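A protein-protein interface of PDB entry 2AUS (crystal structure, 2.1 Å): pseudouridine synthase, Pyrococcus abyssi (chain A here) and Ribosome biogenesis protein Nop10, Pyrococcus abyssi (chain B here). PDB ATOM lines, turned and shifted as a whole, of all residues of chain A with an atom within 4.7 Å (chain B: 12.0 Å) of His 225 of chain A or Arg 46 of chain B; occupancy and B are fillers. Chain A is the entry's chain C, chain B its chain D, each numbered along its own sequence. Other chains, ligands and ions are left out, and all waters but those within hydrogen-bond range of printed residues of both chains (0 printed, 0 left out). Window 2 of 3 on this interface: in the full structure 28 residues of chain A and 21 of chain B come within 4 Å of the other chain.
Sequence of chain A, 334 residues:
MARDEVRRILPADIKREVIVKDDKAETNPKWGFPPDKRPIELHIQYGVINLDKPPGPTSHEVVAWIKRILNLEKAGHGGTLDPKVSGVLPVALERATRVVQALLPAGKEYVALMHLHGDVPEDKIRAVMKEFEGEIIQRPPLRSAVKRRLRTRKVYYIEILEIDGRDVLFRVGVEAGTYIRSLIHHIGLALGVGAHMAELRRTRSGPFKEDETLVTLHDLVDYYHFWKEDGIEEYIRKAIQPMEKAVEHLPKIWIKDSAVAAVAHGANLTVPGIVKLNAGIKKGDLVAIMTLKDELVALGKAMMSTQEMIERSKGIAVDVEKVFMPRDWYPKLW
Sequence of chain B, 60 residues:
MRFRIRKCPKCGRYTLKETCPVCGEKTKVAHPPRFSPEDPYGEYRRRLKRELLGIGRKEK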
ATOM      1  N   VAL A 221       3.513 -11.759 -12.043  1.00  0.00           N
ATOM      2  CA  VAL A 221       2.652 -11.621 -10.876  1.00  0.00           C
ATOM      3  C   VAL A 221       1.808 -10.360 -11.019  1.00  0.00           C
ATOM      4  O   VAL A 221       0.593 -10.399 -10.853  1.00  0.00           O
ATOM      5  CB  VAL A 221       3.472 -11.527  -9.575  1.00  0.00           C
ATOM      6  CG1 VAL A 221       2.561 -11.133  -8.409  1.00  0.00           C
ATOM      7  CG2 VAL A 221       4.153 -12.869  -9.294  1.00  0.00           C
ATOM      8  N   ASP A 222       2.449  -9.249 -11.361  1.00  0.00           N
ATOM      9  CA  ASP A 222       1.728  -7.991 -11.495  1.00  0.00           C
ATOM     10  C   ASP A 222       0.738  -7.946 -12.651  1.00  0.00           C
ATOM     11  O   ASP A 222      -0.367  -7.419 -12.506  1.00  0.00           O
ATOM     12  CB  ASP A 222       2.717  -6.833 -11.612  1.00  0.00           C
ATOM     13  CG  ASP A 222       3.636  -6.736 -10.409  1.00  0.00           C
ATOM     14  OD1 ASP A 222       3.346  -7.395  -9.383  1.00  0.00           O
ATOM     15  OD2 ASP A 222       4.643  -6.000 -10.482  1.00  0.00           O
ATOM     16  N   TYR A 223       1.122  -8.490 -13.800  1.00  0.00           N
ATOM     17  CA  TYR A 223       0.236  -8.489 -14.959  1.00  0.00           C
ATOM     18  C   TYR A 223      -0.972  -9.394 -14.732  1.00  0.00           C
ATOM     19  O   TYR A 223      -2.079  -9.108 -15.195  1.00  0.00           O
ATOM     20  CB  TYR A 223       1.002  -8.950 -16.194  1.00  0.00           C
ATOM     21  CG  TYR A 223       2.151  -8.052 -16.579  1.00  0.00           C
ATOM     22  CD1 TYR A 223       3.146  -8.508 -17.437  1.00  0.00           C
ATOM     23  CD2 TYR A 223       2.225  -6.729 -16.124  1.00  0.00           C
ATOM     24  CE1 TYR A 223       4.186  -7.680 -17.841  1.00  0.00           C
ATOM     25  CE2 TYR A 223       3.261  -5.887 -16.526  1.00  0.00           C
ATOM     26  CZ  TYR A 223       4.240  -6.374 -17.386  1.00  0.00           C
ATOM     27  OH  TYR A 223       5.280  -5.566 -17.787  1.00  0.00           O
ATOM     28  N   TYR A 224      -0.758 -10.487 -14.014  1.00  0.00           N
ATOM     29  CA  TYR A 224      -1.842 -11.409 -13.731  1.00  0.00           C
ATOM     30  C   TYR A 224      -2.825 -10.707 -12.804  1.00  0.00           C
ATOM     31  O   TYR A 224      -4.036 -10.906 -12.907  1.00  0.00           O
ATOM     32  CB  TYR A 224      -1.299 -12.677 -13.083  1.00  0.00           C
ATOM     33  CG  TYR A 224      -2.304 -13.798 -13.033  1.00  0.00           C
ATOM     34  CD1 TYR A 224      -2.918 -14.154 -11.833  1.00  0.00           C
ATOM     35  CD2 TYR A 224      -2.644 -14.503 -14.186  1.00  0.00           C
ATOM     36  CE1 TYR A 224      -3.845 -15.186 -11.777  1.00  0.00           C
ATOM     37  CE2 TYR A 224      -3.569 -15.539 -14.143  1.00  0.00           C
ATOM     38  CZ  TYR A 224      -4.167 -15.875 -12.935  1.00  0.00           C
ATOM     39  OH  TYR A 224      -5.084 -16.897 -12.886  1.00  0.00           O
ATOM     40  N   HIS A 225      -2.289  -9.874 -11.911  1.00  0.00           N
ATOM     41  CA  HIS A 225      -3.106  -9.097 -10.980  1.00  0.00           C
ATOM     42  C   HIS A 225      -3.928  -8.069 -11.753  1.00  0.00           C
ATOM     43  O   HIS A 225      -5.122  -7.917 -11.513  1.00  0.00           O
ATOM     44  CB  HIS A 225      -2.219  -8.375  -9.958  1.00  0.00           C
ATOM     45  CG  HIS A 225      -1.993  -9.149  -8.697  1.00  0.00           C
ATOM     46  ND1 HIS A 225      -2.786  -8.999  -7.579  1.00  0.00           N
ATOM     47  CD2 HIS A 225      -1.079 -10.097  -8.381  1.00  0.00           C
ATOM     48  CE1 HIS A 225      -2.370  -9.817  -6.628  1.00  0.00           C
ATOM     49  NE2 HIS A 225      -1.334 -10.495  -7.089  1.00  0.00           N
ATOM     50  N   PHE A 226      -3.290  -7.369 -12.685  1.00  0.00           N
ATOM     51  CA  PHE A 226      -3.987  -6.362 -13.480  1.00  0.00           C
ATOM     52  C   PHE A 226      -5.129  -7.004 -14.264  1.00  0.00           C
ATOM     53  O   PHE A 226      -6.157  -6.377 -14.515  1.00  0.00           O
ATOM     54  CB  PHE A 226      -3.015  -5.684 -14.451  1.00  0.00           C
ATOM     55  CG  PHE A 226      -1.906  -4.916 -13.776  1.00  0.00           C
ATOM     56  CD1 PHE A 226      -0.781  -4.529 -14.495  1.00  0.00           C
ATOM     57  CD2 PHE A 226      -1.991  -4.571 -12.428  1.00  0.00           C
ATOM     58  CE1 PHE A 226       0.244  -3.809 -13.883  1.00  0.00           C
ATOM     59  CE2 PHE A 226      -0.970  -3.851 -11.805  1.00  0.00           C
ATOM     60  CZ  PHE A 226       0.147  -3.470 -12.534  1.00  0.00           C
ATOM     61  N   TRP A 227      -4.938  -8.257 -14.653  1.00  0.00           N
ATOM     62  CA  TRP A 227      -5.955  -8.979 -15.398  1.00  0.00           C
ATOM     63  C   TRP A 227      -7.075  -9.466 -14.486  1.00  0.00           C
ATOM     64  O   TRP A 227      -8.225  -9.096 -14.662  1.00  0.00           O
ATOM     65  CB  TRP A 227      -5.324 -10.169 -16.136  1.00  0.00           C
ATOM     66  CG  TRP A 227      -6.305 -11.013 -16.881  1.00  0.00           C
ATOM     67  CD1 TRP A 227      -7.394 -10.577 -17.579  1.00  0.00           C
ATOM     68  CD2 TRP A 227      -6.271 -12.438 -17.035  1.00  0.00           C
ATOM     69  NE1 TRP A 227      -8.040 -11.638 -18.157  1.00  0.00           N
ATOM     70  CE2 TRP A 227      -7.376 -12.793 -17.842  1.00  0.00           C
ATOM     71  CE3 TRP A 227      -5.415 -13.447 -16.576  1.00  0.00           C
ATOM     72  CZ2 TRP A 227      -7.651 -14.120 -18.195  1.00  0.00           C
ATOM     73  CZ3 TRP A 227      -5.686 -14.770 -16.930  1.00  0.00           C
ATOM     74  CH2 TRP A 227      -6.798 -15.091 -17.733  1.00  0.00           C
ATOM     75  N   LYS A 228      -6.726 -10.280 -13.498  1.00  0.00           N
ATOM     76  CA  LYS A 228      -7.704 -10.844 -12.580  1.00  0.00           C
ATOM     77  C   LYS A 228      -8.379  -9.893 -11.593  1.00  0.00           C
ATOM     78  O   LYS A 228      -9.529 -10.114 -11.219  1.00  0.00           O
ATOM     79  CB  LYS A 228      -7.073 -12.008 -11.817  1.00  0.00           C
ATOM     80  CG  LYS A 228      -6.826 -13.229 -12.682  1.00  0.00           C
ATOM     81  CD  LYS A 228      -8.129 -13.709 -13.317  1.00  0.00           C
ATOM     82  CE  LYS A 228      -7.903 -14.923 -14.206  1.00  0.00           C
ATOM     83  NZ  LYS A 228      -9.157 -15.318 -14.907  1.00  0.00           N
ATOM     84  N   GLU A 229      -7.683  -8.844 -11.168  1.00  0.00           N
ATOM     85  CA  GLU A 229      -8.275  -7.909 -10.219  1.00  0.00           C
ATOM     86  C   GLU A 229      -8.821  -6.661 -10.893  1.00  0.00           C
ATOM     87  O   GLU A 229      -9.922  -6.221 -10.591  1.00  0.00           O
ATOM     88  CB  GLU A 229      -7.252  -7.468  -9.172  1.00  0.00           C
ATOM     89  CG  GLU A 229      -6.595  -8.575  -8.388  1.00  0.00           C
ATOM     90  CD  GLU A 229      -5.582  -8.037  -7.385  1.00  0.00           C
ATOM     91  OE1 GLU A 229      -4.699  -7.241  -7.792  1.00  0.00           O
ATOM     92  OE2 GLU A 229      -5.674  -8.406  -6.192  1.00  0.00           O
ATOM     93  N   ASP A 230      -8.042  -6.091 -11.802  1.00  0.00           N
ATOM     94  CA  ASP A 230      -8.440  -4.868 -12.483  1.00  0.00           C
ATOM     95  C   ASP A 230      -9.114  -5.065 -13.841  1.00  0.00           C
ATOM     96  O   ASP A 230      -9.556  -4.098 -14.460  1.00  0.00           O
ATOM     97  CB  ASP A 230      -7.217  -3.957 -12.624  1.00  0.00           C
ATOM     98  CG  ASP A 230      -6.516  -3.721 -11.293  1.00  0.00           C
ATOM     99  OD1 ASP A 230      -7.202  -3.322 -10.329  1.00  0.00           O
ATOM    100  OD2 ASP A 230      -5.287  -3.939 -11.202  1.00  0.00           O
ATOM    101  N   PHE B  35      13.476 -14.079  -6.645  1.00  0.00           N
ATOM    102  CA  PHE B  35      12.034 -14.176  -6.468  1.00  0.00           C
ATOM    103  C   PHE B  35      11.712 -14.829  -5.135  1.00  0.00           C
ATOM    104  O   PHE B  35      12.463 -15.678  -4.653  1.00  0.00           O
ATOM    105  CB  PHE B  35      11.405 -14.992  -7.600  1.00  0.00           C
ATOM    106  CG  PHE B  35       9.901 -15.021  -7.564  1.00  0.00           C
ATOM    107  CD1 PHE B  35       9.165 -13.873  -7.841  1.00  0.00           C
ATOM    108  CD2 PHE B  35       9.221 -16.186  -7.229  1.00  0.00           C
ATOM    109  CE1 PHE B  35       7.775 -13.886  -7.790  1.00  0.00           C
ATOM    110  CE2 PHE B  35       7.831 -16.210  -7.174  1.00  0.00           C
ATOM    111  CZ  PHE B  35       7.106 -15.059  -7.451  1.00  0.00           C
ATOM    112  N   SER B  36      10.594 -14.427  -4.541  1.00  0.00           N
ATOM    113  CA  SER B  36      10.158 -14.978  -3.265  1.00  0.00           C
ATOM    114  C   SER B  36       8.636 -15.016  -3.202  1.00  0.00           C
ATOM    115  O   SER B  36       7.964 -14.066  -3.601  1.00  0.00           O
ATOM    116  CB  SER B  36      10.698 -14.135  -2.109  1.00  0.00           C
ATOM    117  OG  SER B  36      10.315 -14.688  -0.862  1.00  0.00           O
ATOM    118  N   PRO B  37       8.072 -16.122  -2.695  1.00  0.00           N
ATOM    119  CA  PRO B  37       6.617 -16.268  -2.586  1.00  0.00           C
ATOM    120  C   PRO B  37       5.973 -15.209  -1.693  1.00  0.00           C
ATOM    121  O   PRO B  37       4.758 -15.003  -1.738  1.00  0.00           O
ATOM    122  CB  PRO B  37       6.458 -17.683  -2.029  1.00  0.00           C
ATOM    123  CG  PRO B  37       7.705 -17.859  -1.209  1.00  0.00           C
ATOM    124  CD  PRO B  37       8.762 -17.290  -2.121  1.00  0.00           C
ATOM    125  N   GLU B  38       6.787 -14.537  -0.882  1.00  0.00           N
ATOM    126  CA  GLU B  38       6.278 -13.501   0.012  1.00  0.00           C
ATOM    127  C   GLU B  38       5.892 -12.262  -0.788  1.00  0.00           C
ATOM    128  O   GLU B  38       4.723 -11.884  -0.834  1.00  0.00           O
ATOM    129  CB  GLU B  38       7.330 -13.131   1.060  1.00  0.00           C
ATOM    130  CG  GLU B  38       7.705 -14.265   2.009  1.00  0.00           C
ATOM    131  CD  GLU B  38       8.630 -13.805   3.127  1.00  0.00           C
ATOM    132  OE1 GLU B  38       9.727 -13.285   2.821  1.00  0.00           O
ATOM    133  OE2 GLU B  38       8.266 -13.968   4.312  1.00  0.00           O
ATOM    134  N   ASP B  39       6.878 -11.629  -1.414  1.00  0.00           N
ATOM    135  CA  ASP B  39       6.626 -10.439  -2.219  1.00  0.00           C
ATOM    136  C   ASP B  39       5.890  -9.365  -1.408  1.00  0.00           C
ATOM    137  O   ASP B  39       4.792  -8.934  -1.766  1.00  0.00           O
ATOM    138  CB  ASP B  39       5.811 -10.831  -3.455  1.00  0.00           C
ATOM    139  CG  ASP B  39       5.778  -9.745  -4.500  1.00  0.00           C
ATOM    140  OD1 ASP B  39       6.829  -9.098  -4.694  1.00  0.00           O
ATOM    141  OD2 ASP B  39       4.708  -9.550  -5.123  1.00  0.00           O
ATOM    142  N   PRO B  40       6.503  -8.910  -0.303  1.00  0.00           N
ATOM    143  CA  PRO B  40       5.954  -7.891   0.599  1.00  0.00           C
ATOM    144  C   PRO B  40       5.631  -6.556  -0.071  1.00  0.00           C
ATOM    145  O   PRO B  40       4.671  -5.883   0.300  1.00  0.00           O
ATOM    146  CB  PRO B  40       7.053  -7.731   1.653  1.00  0.00           C
ATOM    147  CG  PRO B  40       7.761  -9.058   1.624  1.00  0.00           C
ATOM    148  CD  PRO B  40       7.834  -9.338   0.156  1.00  0.00           C
ATOM    149  N   TYR B  41       6.443  -6.179  -1.053  1.00  0.00           N
ATOM    150  CA  TYR B  41       6.260  -4.915  -1.750  1.00  0.00           C
ATOM    151  C   TYR B  41       5.454  -5.044  -3.038  1.00  0.00           C
ATOM    152  O   TYR B  41       5.376  -4.097  -3.826  1.00  0.00           O
ATOM    153  CB  TYR B  41       7.630  -4.296  -2.049  1.00  0.00           C
ATOM    154  CG  TYR B  41       8.441  -4.009  -0.802  1.00  0.00           C
ATOM    155  CD1 TYR B  41       8.162  -2.900  -0.002  1.00  0.00           C
ATOM    156  CD2 TYR B  41       9.467  -4.866  -0.404  1.00  0.00           C
ATOM    157  CE1 TYR B  41       8.886  -2.651   1.162  1.00  0.00           C
ATOM    158  CE2 TYR B  41      10.191  -4.628   0.757  1.00  0.00           C
ATOM    159  CZ  TYR B  41       9.899  -3.520   1.536  1.00  0.00           C
ATOM    160  OH  TYR B  41      10.617  -3.281   2.686  1.00  0.00           O
ATOM    161  N   GLY B  42       4.852  -6.214  -3.241  1.00  0.00           N
ATOM    162  CA  GLY B  42       4.050  -6.441  -4.432  1.00  0.00           C
ATOM    163  C   GLY B  42       3.022  -5.344  -4.649  1.00  0.00           C
ATOM    164  O   GLY B  42       2.913  -4.790  -5.741  1.00  0.00           O
ATOM    165  N   GLU B  43       2.268  -5.019  -3.605  1.00  0.00           N
ATOM    166  CA  GLU B  43       1.255  -3.977  -3.716  1.00  0.00           C
ATOM    167  C   GLU B  43       1.915  -2.642  -4.012  1.00  0.00           C
ATOM    168  O   GLU B  43       1.395  -1.839  -4.784  1.00  0.00           O
ATOM    169  CB  GLU B  43       0.432  -3.888  -2.427  1.00  0.00           C
ATOM    170  CG  GLU B  43      -0.369  -5.156  -2.138  1.00  0.00           C
ATOM    171  CD  GLU B  43      -1.298  -5.016  -0.944  1.00  0.00           C
ATOM    172  OE1 GLU B  43      -2.177  -4.123  -0.971  1.00  0.00           O
ATOM    173  OE2 GLU B  43      -1.153  -5.811   0.015  1.00  0.00           O
ATOM    174  N   TYR B  44       3.077  -2.416  -3.411  1.00  0.00           N
ATOM    175  CA  TYR B  44       3.800  -1.172  -3.622  1.00  0.00           C
ATOM    176  C   TYR B  44       4.270  -1.000  -5.064  1.00  0.00           C
ATOM    177  O   TYR B  44       3.951   0.001  -5.714  1.00  0.00           O
ATOM    178  CB  TYR B  44       5.005  -1.083  -2.679  1.00  0.00           C
ATOM    179  CG  TYR B  44       5.905   0.095  -2.980  1.00  0.00           C
ATOM    180  CD1 TYR B  44       5.420   1.402  -2.914  1.00  0.00           C
ATOM    181  CD2 TYR B  44       7.232  -0.098  -3.362  1.00  0.00           C
ATOM    182  CE1 TYR B  44       6.237   2.489  -3.223  1.00  0.00           C
ATOM    183  CE2 TYR B  44       8.054   0.980  -3.674  1.00  0.00           C
ATOM    184  CZ  TYR B  44       7.550   2.269  -3.603  1.00  0.00           C
ATOM    185  OH  TYR B  44       8.357   3.336  -3.919  1.00  0.00           O
ATOM    186  N   ARG B  45       5.021  -1.968  -5.579  1.00  0.00           N
ATOM    187  CA  ARG B  45       5.503  -1.827  -6.949  1.00  0.00           C
ATOM    188  C   ARG B  45       4.359  -1.838  -7.948  1.00  0.00           C
ATOM    189  O   ARG B  45       4.459  -1.228  -9.011  1.00  0.00           O
ATOM    190  CB  ARG B  45       6.524  -2.913  -7.311  1.00  0.00           C
ATOM    191  CG  ARG B  45       5.951  -4.281  -7.468  1.00  0.00           C
ATOM    192  CD  ARG B  45       6.805  -5.154  -8.393  1.00  0.00           C
ATOM    193  NE  ARG B  45       6.195  -6.472  -8.452  1.00  0.00           N
ATOM    194  CZ  ARG B  45       6.206  -7.327  -7.441  1.00  0.00           C
ATOM    195  NH1 ARG B  45       6.820  -7.002  -6.312  1.00  0.00           N
ATOM    196  NH2 ARG B  45       5.549  -8.474  -7.530  1.00  0.00           N
ATOM    197  N   ARG B  46       3.270  -2.525  -7.618  1.00  0.00           N
ATOM    198  CA  ARG B  46       2.130  -2.545  -8.528  1.00  0.00           C
ATOM    199  C   ARG B  46       1.531  -1.147  -8.611  1.00  0.00           C
ATOM    200  O   ARG B  46       1.040  -0.737  -9.662  1.00  0.00           O
ATOM    201  CB  ARG B  46       1.064  -3.544  -8.069  1.00  0.00           C
ATOM    202  CG  ARG B  46       1.262  -4.936  -8.645  1.00  0.00           C
ATOM    203  CD  ARG B  46       0.023  -5.782  -8.497  1.00  0.00           C
ATOM    204  NE  ARG B  46      -0.169  -6.271  -7.136  1.00  0.00           N
ATOM    205  CZ  ARG B  46       0.633  -7.140  -6.533  1.00  0.00           C
ATOM    206  NH1 ARG B  46       1.694  -7.616  -7.166  1.00  0.00           N
ATOM    207  NH2 ARG B  46       0.362  -7.552  -5.303  1.00  0.00           N
ATOM    208  N   ARG B  47       1.585  -0.411  -7.506  1.00  0.00           N
ATOM    209  CA  ARG B  47       1.048   0.941  -7.486  1.00  0.00           C
ATOM    210  C   ARG B  47       1.918   1.846  -8.355  1.00  0.00           C
ATOM    211  O   ARG B  47       1.426   2.795  -8.964  1.00  0.00           O
ATOM    212  CB  ARG B  47       0.985   1.466  -6.049  1.00  0.00           C
ATOM    213  CG  ARG B  47       0.150   2.728  -5.903  1.00  0.00           C
ATOM    214  CD  ARG B  47      -0.463   2.848  -4.511  1.00  0.00           C
ATOM    215  NE  ARG B  47       0.543   2.827  -3.450  1.00  0.00           N
ATOM    216  CZ  ARG B  47       1.575   3.663  -3.375  1.00  0.00           C
ATOM    217  NH1 ARG B  47       1.754   4.595  -4.304  1.00  0.00           N
ATOM    218  NH2 ARG B  47       2.430   3.574  -2.362  1.00  0.00           N
ATOM    219  N   LEU B  48       3.211   1.543  -8.417  1.00  0.00           N
ATOM    220  CA  LEU B  48       4.138   2.320  -9.233  1.00  0.00           C
ATOM    221  C   LEU B  48       3.862   2.065 -10.714  1.00  0.00           C
ATOM    222  O   LEU B  48       3.944   2.977 -11.537  1.00  0.00           O
ATOM    223  CB  LEU B  48       5.587   1.946  -8.901  1.00  0.00           C
ATOM    224  CG  LEU B  48       6.109   2.359  -7.518  1.00  0.00           C
ATOM    225  CD1 LEU B  48       7.480   1.733  -7.272  1.00  0.00           C
ATOM    226  CD2 LEU B  48       6.186   3.882  -7.435  1.00  0.00           C
ATOM    227  N   LYS B  49       3.540   0.818 -11.050  1.00  0.00           N
ATOM    228  CA  LYS B  49       3.236   0.446 -12.430  1.00  0.00           C
ATOM    229  C   LYS B  49       1.822   0.907 -12.758  1.00  0.00           C
ATOM    230  O   LYS B  49       1.584   1.559 -13.773  1.00  0.00           O
ATOM    231  CB  LYS B  49       3.318  -1.072 -12.610  1.00  0.00           C
ATOM    232  CG  LYS B  49       4.661  -1.675 -12.248  1.00  0.00           C
ATOM    233  CD  LYS B  49       4.670  -3.179 -12.479  1.00  0.00           C
ATOM    234  CE  LYS B  49       6.043  -3.772 -12.192  1.00  0.00           C
ATOM    235  NZ  LYS B  49       6.100  -5.242 -12.447  1.00  0.00           N
ATOM    236  N   ARG B  50       0.892   0.558 -11.876  1.00  0.00           N
ATOM    237  CA  ARG B  50      -0.515   0.905 -12.026  1.00  0.00           C
ATOM    238  C   ARG B  50      -0.667   2.413 -12.195  1.00  0.00           C
ATOM    239  O   ARG B  50      -1.731   2.905 -12.573  1.00  0.00           O
ATOM    240  CB  ARG B  50      -1.283   0.419 -10.795  1.00  0.00           C
ATOM    241  CG  ARG B  50      -2.787   0.435 -10.910  1.00  0.00           C
ATOM    242  CD  ARG B  50      -3.391  -0.317  -9.740  1.00  0.00           C
ATOM    243  NE  ARG B  50      -3.141  -1.754  -9.822  1.00  0.00           N
ATOM    244  CZ  ARG B  50      -2.970  -2.543  -8.767  1.00  0.00           C
ATOM    245  NH1 ARG B  50      -3.012  -2.038  -7.542  1.00  0.00           N
ATOM    246  NH2 ARG B  50      -2.774  -3.844  -8.932  1.00  0.00           N
ATOM    247  N   GLU B  51       0.411   3.140 -11.920  1.00  0.00           N
ATOM    248  CA  GLU B  51       0.419   4.592 -12.044  1.00  0.00           C
ATOM    249  C   GLU B  51       1.284   5.006 -13.230  1.00  0.00           C
ATOM    250  O   GLU B  51       1.039   6.034 -13.861  1.00  0.00           O
ATOM    251  CB  GLU B  51       0.965   5.228 -10.766  1.00  0.00           C
ATOM    252  CG  GLU B  51       1.001   6.746 -10.803  1.00  0.00           C
ATOM    253  CD  GLU B  51       1.745   7.337  -9.622  1.00  0.00           C
ATOM    254  OE1 GLU B  51       1.327   7.095  -8.468  1.00  0.00           O
ATOM    255  OE2 GLU B  51       2.752   8.044  -9.852  1.00  0.00           O
ATOM    256  N   LEU B  52       2.302   4.205 -13.525  1.00  0.00           N
ATOM    257  CA  LEU B  52       3.194   4.491 -14.640  1.00  0.00           C
ATOM    258  C   LEU B  52       2.541   4.050 -15.949  1.00  0.00           C
ATOM    259  O   LEU B  52       2.972   4.436 -17.036  1.00  0.00           O
ATOM    260  CB  LEU B  52       4.533   3.772 -14.435  1.00  0.00           C
ATOM    261  CG  LEU B  52       5.618   3.910 -15.509  1.00  0.00           C
ATOM    262  CD1 LEU B  52       6.988   3.733 -14.873  1.00  0.00           C
ATOM    263  CD2 LEU B  52       5.394   2.886 -16.614  1.00  0.00           C
ATOM    264  N   LEU B  53       1.493   3.242 -15.832  1.00  0.00           N
ATOM    265  CA  LEU B  53       0.768   2.751 -16.998  1.00  0.00           C
ATOM    266  C   LEU B  53      -0.586   3.447 -17.075  1.00  0.00           C
ATOM    267  O   LEU B  53      -1.238   3.452 -18.120  1.00  0.00           O
ATOM    268  CB  LEU B  53       0.569   1.234 -16.897  1.00  0.00           C
ATOM    269  CG  LEU B  53       1.837   0.378 -16.811  1.00  0.00           C
ATOM    270  CD1 LEU B  53       1.460  -1.076 -16.602  1.00  0.00           C
ATOM    271  CD2 LEU B  53       2.658   0.539 -18.078  1.00  0.00           C
ATOM    272  N   GLY B  54      -1.001   4.036 -15.958  1.00  0.00           N
ATOM    273  CA  GLY B  54      -2.276   4.727 -15.912  1.00  0.00           C
ATOM    274  C   GLY B  54      -3.430   3.754 -15.772  1.00  0.00           C
ATOM    275  O   GLY B  54      -4.101   3.433 -16.751  1.00  0.00           O
ATOM    276  N   ILE B  55      -3.665   3.283 -14.552  1.00  0.00           N
ATOM    277  CA  ILE B  55      -4.742   2.336 -14.302  1.00  0.00           C
ATOM    278  C   ILE B  55      -5.609   2.767 -13.118  1.00  0.00           C
ATOM    279  O   ILE B  55      -6.803   2.466 -13.068  1.00  0.00           O
ATOM    280  CB  ILE B  55      -4.171   0.922 -14.035  1.00  0.00           C
ATOM    281  CG1 ILE B  55      -3.287   0.491 -15.209  1.00  0.00           C
ATOM    282  CG2 ILE B  55      -5.307  -0.074 -13.832  1.00  0.00           C
ATOM    283  CD1 ILE B  55      -2.616  -0.854 -15.019  1.00  0.00           C
ATOM    284  N   GLY B  56      -5.004   3.477 -12.171  1.00  0.00           N
ATOM    285  CA  GLY B  56      -5.738   3.934 -11.005  1.00  0.00           C
ATOM    286  C   GLY B  56      -5.326   3.209  -9.739  1.00  0.00           C
ATOM    287  O   GLY B  56      -5.802   3.523  -8.646  1.00  0.00           O
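Of chain B, only Arg 45 (2.6 Å), Arg 46 (2.8 Å) and Lys 49 (2.6 Å) come within 4 Å of Asp 222 of chain A.
Asp 230 of chain A touches one residue of chain B.
Of the printed residues of chain A, Arg 45 of chain B touches Asp 222.
Of chain A, only Val 221, Asp 222, His 225 and Phe 226 come within 4 Å of Arg 46 of chain B.
Printed residues of chain A within 4 Å of Lys 49 of chain B: Asp 222 and Phe 226.
Of the printed residues of chain A, Arg 50 of chain B touches Phe 226 and Asp 230.
NE of Arg 45 of chain B lies within salt-bridge range of OD2 of Asp 222 of chain A.
OD1 of Asp 222 of chain A lies within salt-bridge range of NH1 of Arg 46 of chain B (2.8 Å).
The side-chain amino group (NZ) of Lys 49 of chain B is in salt-bridge range of the side-chain carboxylate (OD2) of Asp 222 of chain A (2.6 Å).
OD2 of Asp 230 of chain A lies within salt-bridge range of NE of Arg 50 of chain B (3.4 Å).
Val 221 of chain A touches Arg 46 of chain B.
CB of His 225 of chain A touches CD of Arg 46 of chain B, at 3.7 Å.
Phe 226 of chain A touches Arg 46 of chain B.
Phe 226 of chain A touches Lys 49 of chain B (CZ to CB, 3.98 Å).
Arg 50 of chain B touches Phe 226 of chain A (NH2 to CE2, 3.4 Å).
OE1 of Glu 229 of chain A lies within hydrogen-bond range of ND1 of His 225 of chain A (2.6 Å).
The backbone carbonyl oxygen of His 225 of chain A lies within hydrogen-bond range of the backbone NH of Asp 230 of chain A, 3.5 Å away.
NH1 of Arg 45 of chain B lies within salt-bridge range of OD1 of Asp 39 of chain B (2.6 Å).
The backbone carbonyl oxygen (O) of Gly 42 of chain B sits close to the guanidinium group (NH1) of Arg 46 of chain B, 3.4 Å away.
The backbone NH (N) of Ile 55 of chain B lies within hydrogen-bond range of the backbone carbonyl oxygen (O) of Arg 50 of chain B.
The backbone carbonyl oxygen of Arg 50 of chain B is in hydrogen-bond range of the backbone NH of Gly 56 of chain B, 3.3 Å away.
Printed residues of chain B that touch a printed residue of chain A: Arg 45, Arg 46, Lys 49 and Arg 50.
Of the 10 printed residues of chain A, 5 touch a printed residue of chain B.
Printed residues of chain A that touch a printed residue of chain B: Val 221, Asp 222, His 225, Phe 226 and Asp 230.
Hydrophobic or aromatic side chains of chain A within 4 Å of the printed part of chain B: Val 221, His 225 and Phe 226.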
